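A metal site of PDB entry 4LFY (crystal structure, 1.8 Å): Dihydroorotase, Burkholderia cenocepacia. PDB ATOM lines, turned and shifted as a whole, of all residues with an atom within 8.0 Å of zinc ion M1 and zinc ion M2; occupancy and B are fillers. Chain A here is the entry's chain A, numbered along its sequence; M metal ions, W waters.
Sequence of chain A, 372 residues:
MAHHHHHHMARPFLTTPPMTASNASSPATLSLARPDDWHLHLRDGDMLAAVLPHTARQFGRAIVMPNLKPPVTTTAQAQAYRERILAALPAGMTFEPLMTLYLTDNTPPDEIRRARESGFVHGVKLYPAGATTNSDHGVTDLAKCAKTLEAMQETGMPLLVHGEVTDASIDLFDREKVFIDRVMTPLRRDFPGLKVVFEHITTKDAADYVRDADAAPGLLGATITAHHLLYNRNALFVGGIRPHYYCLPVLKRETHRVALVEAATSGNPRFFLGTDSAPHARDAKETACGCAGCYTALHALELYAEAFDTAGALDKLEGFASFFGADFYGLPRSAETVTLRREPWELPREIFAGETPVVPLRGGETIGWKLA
NE2 of His 162 is in hydrogen-bond range of OE1 of Glu 164 (2.8 Å).
NZ of KCX 125 sits at hydrogen-bond distance from the side-chain sulfur (SD) of Met 65, 3.6 Å away.
The backbone carbonyl oxygen of Ser 277 sits at hydrogen-bond distance from the backbone NH of His 41 (3.2 Å).
The backbone carbonyl oxygen of His 39 sits at hydrogen-bond distance from the side-chain hydroxyl of Thr 275 (3.4 Å).
NZ of KCX 125 is in hydrogen-bond range of OH of Tyr 127 (3.2 Å).
N of His 162 is in hydrogen-bond range of O of Leu 126, 3.0 Å away.
A ring nitrogen (ND1) of His 39 sits at hydrogen-bond distance from the side-chain carboxylate (OE1) of Glu 199, at 2.7 Å.
The side-chain amide oxygen of Asn 67 is in hydrogen-bond range of a ring nitrogen (ND1) of His 41 (2.8 Å).
Within 4 Å of zinc ion M1: His 39, KCX 125, His 162 and His 200.
The nearest printed residue that does not touch zinc ion M1 is Leu 248 (4.4 Å).
Of the 24 residues printed, 4 come within 4 Å of zinc ion M2.
The nearest printed residue that does not touch zinc ion M2 is His 200 (4.2 Å).
OQ2 of KCX 125 is bound to zinc ion M1, 1.8 Å away.
NE2 of His 200 is bound to zinc ion M1 (2.1 Å).
Zinc ion M1 is bound by water W1.
Zinc ion M1 is bound by ND1 of His 162 (2.2 Å).
Zinc ion M1 has four donor atoms within binding distance.
Zinc ion M2 is bound by water W1, OQ1 of KCX 125, a ring nitrogen (NE2) of His 41, the side-chain carboxylate (OD1) of Asp 276 and a ring nitrogen (NE2) of His 39.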
ATOM      1  N   HIS A  39     -27.204  10.284 -16.252  1.00  0.00           N
ATOM      2  CA  HIS A  39     -27.266  11.665 -15.747  1.00  0.00           C
ATOM      3  C   HIS A  39     -28.635  12.273 -15.990  1.00  0.00           C
ATOM      4  O   HIS A  39     -28.892  12.734 -17.086  1.00  0.00           O
ATOM      5  CB  HIS A  39     -26.185  12.532 -16.424  1.00  0.00           C
ATOM      6  CG  HIS A  39     -26.061  13.938 -15.912  1.00  0.00           C
ATOM      7  ND1 HIS A  39     -24.832  14.513 -15.616  1.00  0.00           N
ATOM      8  CD2 HIS A  39     -26.991  14.883 -15.595  1.00  0.00           C
ATOM      9  CE1 HIS A  39     -25.025  15.749 -15.174  1.00  0.00           C
ATOM     10  NE2 HIS A  39     -26.320  16.002 -15.189  1.00  0.00           N
ATOM     11  N   LEU A  40     -29.494  12.276 -14.991  1.00  0.00           N
ATOM     12  CA  LEU A  40     -30.886  12.668 -15.162  1.00  0.00           C
ATOM     13  C   LEU A  40     -31.385  13.604 -14.082  1.00  0.00           C
ATOM     14  O   LEU A  40     -31.058  13.422 -12.897  1.00  0.00           O
ATOM     15  CB  LEU A  40     -31.726  11.410 -15.225  1.00  0.00           C
ATOM     16  CG  LEU A  40     -33.260  11.578 -15.330  1.00  0.00           C
ATOM     17  CD1 LEU A  40     -33.643  12.162 -16.665  1.00  0.00           C
ATOM     18  CD2 LEU A  40     -33.925  10.218 -15.166  1.00  0.00           C
ATOM     19  N   HIS A  41     -32.168  14.590 -14.498  1.00  0.00           N
ATOM     20  CA  HIS A  41     -32.963  15.434 -13.590  1.00  0.00           C
ATOM     21  C   HIS A  41     -34.432  15.074 -13.642  1.00  0.00           C
ATOM     22  O   HIS A  41     -35.104  15.371 -14.632  1.00  0.00           O
ATOM     23  CB  HIS A  41     -32.754  16.900 -13.950  1.00  0.00           C
ATOM     24  CG  HIS A  41     -31.316  17.322 -13.830  1.00  0.00           C
ATOM     25  ND1 HIS A  41     -30.771  17.730 -12.629  1.00  0.00           N
ATOM     26  CD2 HIS A  41     -30.279  17.271 -14.701  1.00  0.00           C
ATOM     27  CE1 HIS A  41     -29.469  17.983 -12.799  1.00  0.00           C
ATOM     28  NE2 HIS A  41     -29.160  17.692 -14.035  1.00  0.00           N
ATOM     29  N   ARG A  43     -36.592  16.157 -11.184  1.00  0.00           N
ATOM     30  CA  ARG A  43     -37.338  17.207 -10.427  1.00  0.00           C
ATOM     31  C   ARG A  43     -38.216  16.573  -9.322  1.00  0.00           C
ATOM     32  O   ARG A  43     -37.878  15.499  -8.799  1.00  0.00           O
ATOM     33  CB  ARG A  43     -38.196  18.074 -11.375  1.00  0.00           C
ATOM     34  CG  ARG A  43     -37.459  18.542 -12.625  1.00  0.00           C
ATOM     35  CD  ARG A  43     -36.240  19.379 -12.283  1.00  0.00           C
ATOM     36  NE  ARG A  43     -35.718  20.091 -13.480  1.00  0.00           N
ATOM     37  CZ  ARG A  43     -34.499  20.576 -13.602  1.00  0.00           C
ATOM     38  NH1 ARG A  43     -33.607  20.477 -12.631  1.00  0.00           N
ATOM     39  NH2 ARG A  43     -34.153  21.215 -14.688  1.00  0.00           N
ATOM     40  N   MET A  65     -30.085  13.083 -10.298  1.00  0.00           N
ATOM     41  CA  MET A  65     -29.269  14.185  -9.771  1.00  0.00           C
ATOM     42  C   MET A  65     -29.960  14.867  -8.570  1.00  0.00           C
ATOM     43  O   MET A  65     -31.169  14.706  -8.387  1.00  0.00           O
ATOM     44  CB  MET A  65     -28.919  15.177 -10.892  1.00  0.00           C
ATOM     45  CG  MET A  65     -27.873  14.666 -11.847  1.00  0.00           C
ATOM     46  SD  MET A  65     -26.333  14.113 -11.050  1.00  0.00           S
ATOM     47  CE  MET A  65     -25.327  13.488 -12.462  1.00  0.00           C
ATOM     48  N   PRO A  66     -29.163  15.509  -7.699  1.00  0.00           N
ATOM     49  CA  PRO A  66     -29.671  15.929  -6.391  1.00  0.00           C
ATOM     50  C   PRO A  66     -30.028  17.408  -6.232  1.00  0.00           C
ATOM     51  O   PRO A  66     -30.260  17.851  -5.079  1.00  0.00           O
ATOM     52  CB  PRO A  66     -28.451  15.646  -5.479  1.00  0.00           C
ATOM     53  CG  PRO A  66     -27.295  16.005  -6.353  1.00  0.00           C
ATOM     54  CD  PRO A  66     -27.692  15.690  -7.772  1.00  0.00           C
ATOM     55  N   ASN A  67     -30.045  18.133  -7.354  1.00  0.00           N
ATOM     56  CA  ASN A  67     -30.257  19.587  -7.338  1.00  0.00           C
ATOM     57  C   ASN A  67     -31.735  20.013  -7.258  1.00  0.00           C
ATOM     58  O   ASN A  67     -32.185  20.861  -8.030  1.00  0.00           O
ATOM     59  CB  ASN A  67     -29.578  20.229  -8.530  1.00  0.00           C
ATOM     60  CG  ASN A  67     -30.231  19.857  -9.842  1.00  0.00           C
ATOM     61  OD1 ASN A  67     -30.751  18.757  -9.996  1.00  0.00           O
ATOM     62  ND2 ASN A  67     -30.145  20.760 -10.830  1.00  0.00           N
ATOM     63  N   KCX A 125     -22.417  14.339  -6.312  1.00  0.00           N
ATOM     64  CA  KCX A 125     -22.255  15.328  -7.385  1.00  0.00           C
ATOM     65  CB  KCX A 125     -23.647  15.686  -7.852  1.00  0.00           C
ATOM     66  CG  KCX A 125     -23.715  16.712  -8.957  1.00  0.00           C
ATOM     67  CD  KCX A 125     -23.073  16.153 -10.267  1.00  0.00           C
ATOM     68  CE  KCX A 125     -23.268  17.020 -11.484  1.00  0.00           C
ATOM     69  NZ  KCX A 125     -24.697  17.178 -11.780  1.00  0.00           N
ATOM     70  C   KCX A 125     -21.626  16.609  -6.913  1.00  0.00           C
ATOM     71  O   KCX A 125     -22.110  17.237  -5.940  1.00  0.00           O
ATOM     72  CX  KCX A 125     -25.089  17.935 -12.803  1.00  0.00           C
ATOM     73  OQ1 KCX A 125     -26.301  18.141 -13.068  1.00  0.00           O
ATOM     74  OQ2 KCX A 125     -24.114  18.509 -13.588  1.00  0.00           O
ATOM     75  N   LEU A 126     -20.626  17.061  -7.659  1.00  0.00           N
ATOM     76  CA  LEU A 126     -19.961  18.346  -7.447  1.00  0.00           C
ATOM     77  C   LEU A 126     -20.433  19.354  -8.510  1.00  0.00           C
ATOM     78  O   LEU A 126     -20.254  19.180  -9.736  1.00  0.00           O
ATOM     79  CB  LEU A 126     -18.430  18.159  -7.574  1.00  0.00           C
ATOM     80  CG  LEU A 126     -17.614  19.490  -7.652  1.00  0.00           C
ATOM     81  CD1 LEU A 126     -17.818  20.315  -6.416  1.00  0.00           C
ATOM     82  CD2 LEU A 126     -16.152  19.229  -7.903  1.00  0.00           C
ATOM     83  N   TYR A 127     -21.089  20.419  -8.030  1.00  0.00           N
ATOM     84  CA  TYR A 127     -21.494  21.517  -8.907  1.00  0.00           C
ATOM     85  C   TYR A 127     -20.622  22.761  -8.682  1.00  0.00           C
ATOM     86  O   TYR A 127     -20.298  23.043  -7.562  1.00  0.00           O
ATOM     87  CB  TYR A 127     -22.903  21.971  -8.586  1.00  0.00           C
ATOM     88  CG  TYR A 127     -23.990  21.101  -9.054  1.00  0.00           C
ATOM     89  CD1 TYR A 127     -24.475  21.197 -10.378  1.00  0.00           C
ATOM     90  CD2 TYR A 127     -24.593  20.198  -8.176  1.00  0.00           C
ATOM     91  CE1 TYR A 127     -25.517  20.364 -10.796  1.00  0.00           C
ATOM     92  CE2 TYR A 127     -25.602  19.338  -8.607  1.00  0.00           C
ATOM     93  CZ  TYR A 127     -26.098  19.427  -9.887  1.00  0.00           C
ATOM     94  OH  TYR A 127     -27.134  18.540 -10.243  1.00  0.00           O
ATOM     95  N   PRO A 128     -20.328  23.533  -9.728  1.00  0.00           N
ATOM     96  CA  PRO A 128     -19.680  24.825  -9.437  1.00  0.00           C
ATOM     97  C   PRO A 128     -20.507  25.664  -8.462  1.00  0.00           C
ATOM     98  O   PRO A 128     -21.712  25.604  -8.495  1.00  0.00           O
ATOM     99  CB  PRO A 128     -19.644  25.544 -10.796  1.00  0.00           C
ATOM    100  CG  PRO A 128     -20.357  24.683 -11.794  1.00  0.00           C
ATOM    101  CD  PRO A 128     -21.012  23.528 -11.044  1.00  0.00           C
ATOM    102  N   VAL A 161     -18.784  15.054 -11.617  1.00  0.00           N
ATOM    103  CA  VAL A 161     -18.337  16.446 -11.714  1.00  0.00           C
ATOM    104  C   VAL A 161     -18.969  17.219 -12.866  1.00  0.00           C
ATOM    105  O   VAL A 161     -18.840  16.819 -14.046  1.00  0.00           O
ATOM    106  CB  VAL A 161     -16.818  16.423 -11.885  1.00  0.00           C
ATOM    107  CG1 VAL A 161     -16.298  17.797 -12.134  1.00  0.00           C
ATOM    108  CG2 VAL A 161     -16.182  15.786 -10.639  1.00  0.00           C
ATOM    109  N   HIS A 162     -19.585  18.359 -12.524  1.00  0.00           N
ATOM    110  CA  HIS A 162     -19.975  19.350 -13.520  1.00  0.00           C
ATOM    111  C   HIS A 162     -18.765  20.239 -13.652  1.00  0.00           C
ATOM    112  O   HIS A 162     -18.525  21.112 -12.797  1.00  0.00           O
ATOM    113  CB  HIS A 162     -21.225  20.129 -13.054  1.00  0.00           C
ATOM    114  CG  HIS A 162     -21.663  21.198 -14.012  1.00  0.00           C
ATOM    115  ND1 HIS A 162     -22.897  21.240 -14.601  1.00  0.00           N
ATOM    116  CD2 HIS A 162     -20.975  22.236 -14.524  1.00  0.00           C
ATOM    117  CE1 HIS A 162     -22.980  22.285 -15.386  1.00  0.00           C
ATOM    118  NE2 HIS A 162     -21.821  22.900 -15.382  1.00  0.00           N
ATOM    119  N   GLY A 163     -17.958  19.979 -14.695  1.00  0.00           N
ATOM    120  CA  GLY A 163     -16.620  20.505 -14.786  1.00  0.00           C
ATOM    121  C   GLY A 163     -16.581  21.832 -15.520  1.00  0.00           C
ATOM    122  O   GLY A 163     -16.136  21.896 -16.672  1.00  0.00           O
ATOM    123  N   GLU A 164     -17.061  22.870 -14.857  1.00  0.00           N
ATOM    124  CA  GLU A 164     -16.831  24.275 -15.298  1.00  0.00           C
ATOM    125  C   GLU A 164     -16.379  25.160 -14.158  1.00  0.00           C
ATOM    126  O   GLU A 164     -16.970  25.070 -13.045  1.00  0.00           O
ATOM    127  CB  GLU A 164     -18.115  24.850 -15.856  1.00  0.00           C
ATOM    128  CG  GLU A 164     -18.591  24.204 -17.124  1.00  0.00           C
ATOM    129  CD  GLU A 164     -19.803  24.874 -17.696  1.00  0.00           C
ATOM    130  OE1 GLU A 164     -20.884  24.847 -17.100  1.00  0.00           O
ATOM    131  OE2 GLU A 164     -19.637  25.507 -18.735  1.00  0.00           O
ATOM    132  N   GLU A 199     -18.994  14.744 -16.108  1.00  0.00           N
ATOM    133  CA  GLU A 199     -20.353  14.748 -16.650  1.00  0.00           C
ATOM    134  C   GLU A 199     -20.463  15.587 -17.884  1.00  0.00           C
ATOM    135  O   GLU A 199     -19.760  16.598 -18.003  1.00  0.00           O
ATOM    136  CB  GLU A 199     -21.373  15.203 -15.655  1.00  0.00           C
ATOM    137  CG  GLU A 199     -21.437  14.313 -14.434  1.00  0.00           C
ATOM    138  CD  GLU A 199     -21.997  12.898 -14.713  1.00  0.00           C
ATOM    139  OE1 GLU A 199     -22.748  12.745 -15.683  1.00  0.00           O
ATOM    140  OE2 GLU A 199     -21.713  11.987 -13.896  1.00  0.00           O
ATOM    141  N   HIS A 200     -21.420  15.200 -18.720  1.00  0.00           N
ATOM    142  CA  HIS A 200     -21.814  15.904 -19.951  1.00  0.00           C
ATOM    143  C   HIS A 200     -20.647  16.703 -20.534  1.00  0.00           C
ATOM    144  O   HIS A 200     -20.675  17.946 -20.552  1.00  0.00           O
ATOM    145  CB  HIS A 200     -23.010  16.812 -19.707  1.00  0.00           C
ATOM    146  CG  HIS A 200     -22.948  17.644 -18.460  1.00  0.00           C
ATOM    147  ND1 HIS A 200     -21.870  18.435 -18.119  1.00  0.00           N
ATOM    148  CD2 HIS A 200     -23.882  17.881 -17.513  1.00  0.00           C
ATOM    149  CE1 HIS A 200     -22.103  19.043 -16.967  1.00  0.00           C
ATOM    150  NE2 HIS A 200     -23.332  18.733 -16.583  1.00  0.00           N
ATOM    151  N   THR A 225     -24.418  13.846 -23.649  1.00  0.00           N
ATOM    152  CA  THR A 225     -25.866  14.069 -23.886  1.00  0.00           C
ATOM    153  C   THR A 225     -26.197  13.868 -25.369  1.00  0.00           C
ATOM    154  O   THR A 225     -25.308  13.844 -26.212  1.00  0.00           O
ATOM    155  CB  THR A 225     -26.284  15.497 -23.498  1.00  0.00           C
ATOM    156  OG1 THR A 225     -25.750  16.389 -24.464  1.00  0.00           O
ATOM    157  CG2 THR A 225     -25.756  15.896 -22.089  1.00  0.00           C
ATOM    158  N   LEU A 248     -26.569  24.073 -19.612  1.00  0.00           N
ATOM    159  CA  LEU A 248     -25.151  24.100 -19.161  1.00  0.00           C
ATOM    160  C   LEU A 248     -24.629  22.628 -19.138  1.00  0.00           C
ATOM    161  O   LEU A 248     -25.341  21.698 -18.792  1.00  0.00           O
ATOM    162  CB  LEU A 248     -25.007  24.749 -17.795  1.00  0.00           C
ATOM    163  CG  LEU A 248     -25.479  26.211 -17.763  1.00  0.00           C
ATOM    164  CD1 LEU A 248     -25.360  26.675 -16.328  1.00  0.00           C
ATOM    165  CD2 LEU A 248     -24.752  27.177 -18.670  1.00  0.00           C
ATOM    166  N   PRO A 249     -23.437  22.400 -19.639  1.00  0.00           N
ATOM    167  CA  PRO A 249     -22.622  23.388 -20.304  1.00  0.00           C
ATOM    168  C   PRO A 249     -23.191  23.751 -21.670  1.00  0.00           C
ATOM    169  O   PRO A 249     -23.881  22.960 -22.327  1.00  0.00           O
ATOM    170  CB  PRO A 249     -21.247  22.702 -20.402  1.00  0.00           C
ATOM    171  CG  PRO A 249     -21.343  21.423 -19.669  1.00  0.00           C
ATOM    172  CD  PRO A 249     -22.796  21.078 -19.681  1.00  0.00           C
ATOM    173  N   THR A 275     -28.298  11.720 -20.335  1.00  0.00           N
ATOM    174  CA  THR A 275     -29.078  12.686 -21.112  1.00  0.00           C
ATOM    175  C   THR A 275     -28.905  14.116 -20.648  1.00  0.00           C
ATOM    176  O   THR A 275     -29.027  15.040 -21.434  1.00  0.00           O
ATOM    177  CB  THR A 275     -30.597  12.420 -21.064  1.00  0.00           C
ATOM    178  OG1 THR A 275     -31.067  12.455 -19.700  1.00  0.00           O
ATOM    179  CG2 THR A 275     -30.920  11.093 -21.685  1.00  0.00           C
ATOM    180  N   ASP A 276     -28.682  14.293 -19.348  1.00  0.00           N
ATOM    181  CA  ASP A 276     -28.870  15.559 -18.703  1.00  0.00           C
ATOM    182  C   ASP A 276     -30.251  16.172 -19.060  1.00  0.00           C
ATOM    183  O   ASP A 276     -30.380  17.401 -19.149  1.00  0.00           O
ATOM    184  CB  ASP A 276     -27.735  16.562 -19.019  1.00  0.00           C
ATOM    185  CG  ASP A 276     -27.661  17.691 -18.000  1.00  0.00           C
ATOM    186  OD1 ASP A 276     -28.076  17.522 -16.848  1.00  0.00           O
ATOM    187  OD2 ASP A 276     -27.149  18.754 -18.390  1.00  0.00           O
ATOM    188  N   SER A 277     -31.261  15.349 -19.232  1.00  0.00           N
ATOM    189  CA  SER A 277     -32.609  15.824 -19.471  1.00  0.00           C
ATOM    190  C   SER A 277     -33.000  16.650 -18.209  1.00  0.00           C
ATOM    191  O   SER A 277     -32.867  16.197 -17.121  1.00  0.00           O
ATOM    192  CB  SER A 277     -33.598  14.667 -19.640  1.00  0.00           C
ATOM    193  OG  SER A 277     -34.933  15.207 -19.801  1.00  0.00           O
ATOM    194  N   ALA A 278     -33.468  17.882 -18.419  1.00  0.00           N
ATOM    195  CA  ALA A 278     -33.482  18.929 -17.394  1.00  0.00           C
ATOM    196  C   ALA A 278     -34.693  19.837 -17.640  1.00  0.00           C
ATOM    197  O   ALA A 278     -34.548  20.951 -18.183  1.00  0.00           O
ATOM    198  CB  ALA A 278     -32.179  19.705 -17.414  1.00  0.00           C
HETATM  199 ZN    ZN M   1     -24.318  19.637 -15.028  1.00  0.00          ZN
HETATM  200 ZN    ZN M   2     -27.247  17.924 -14.924  1.00  0.00          ZN
HETATM  201  O   HOH W   1     -26.286  19.512 -15.620  1.00  0.00           O
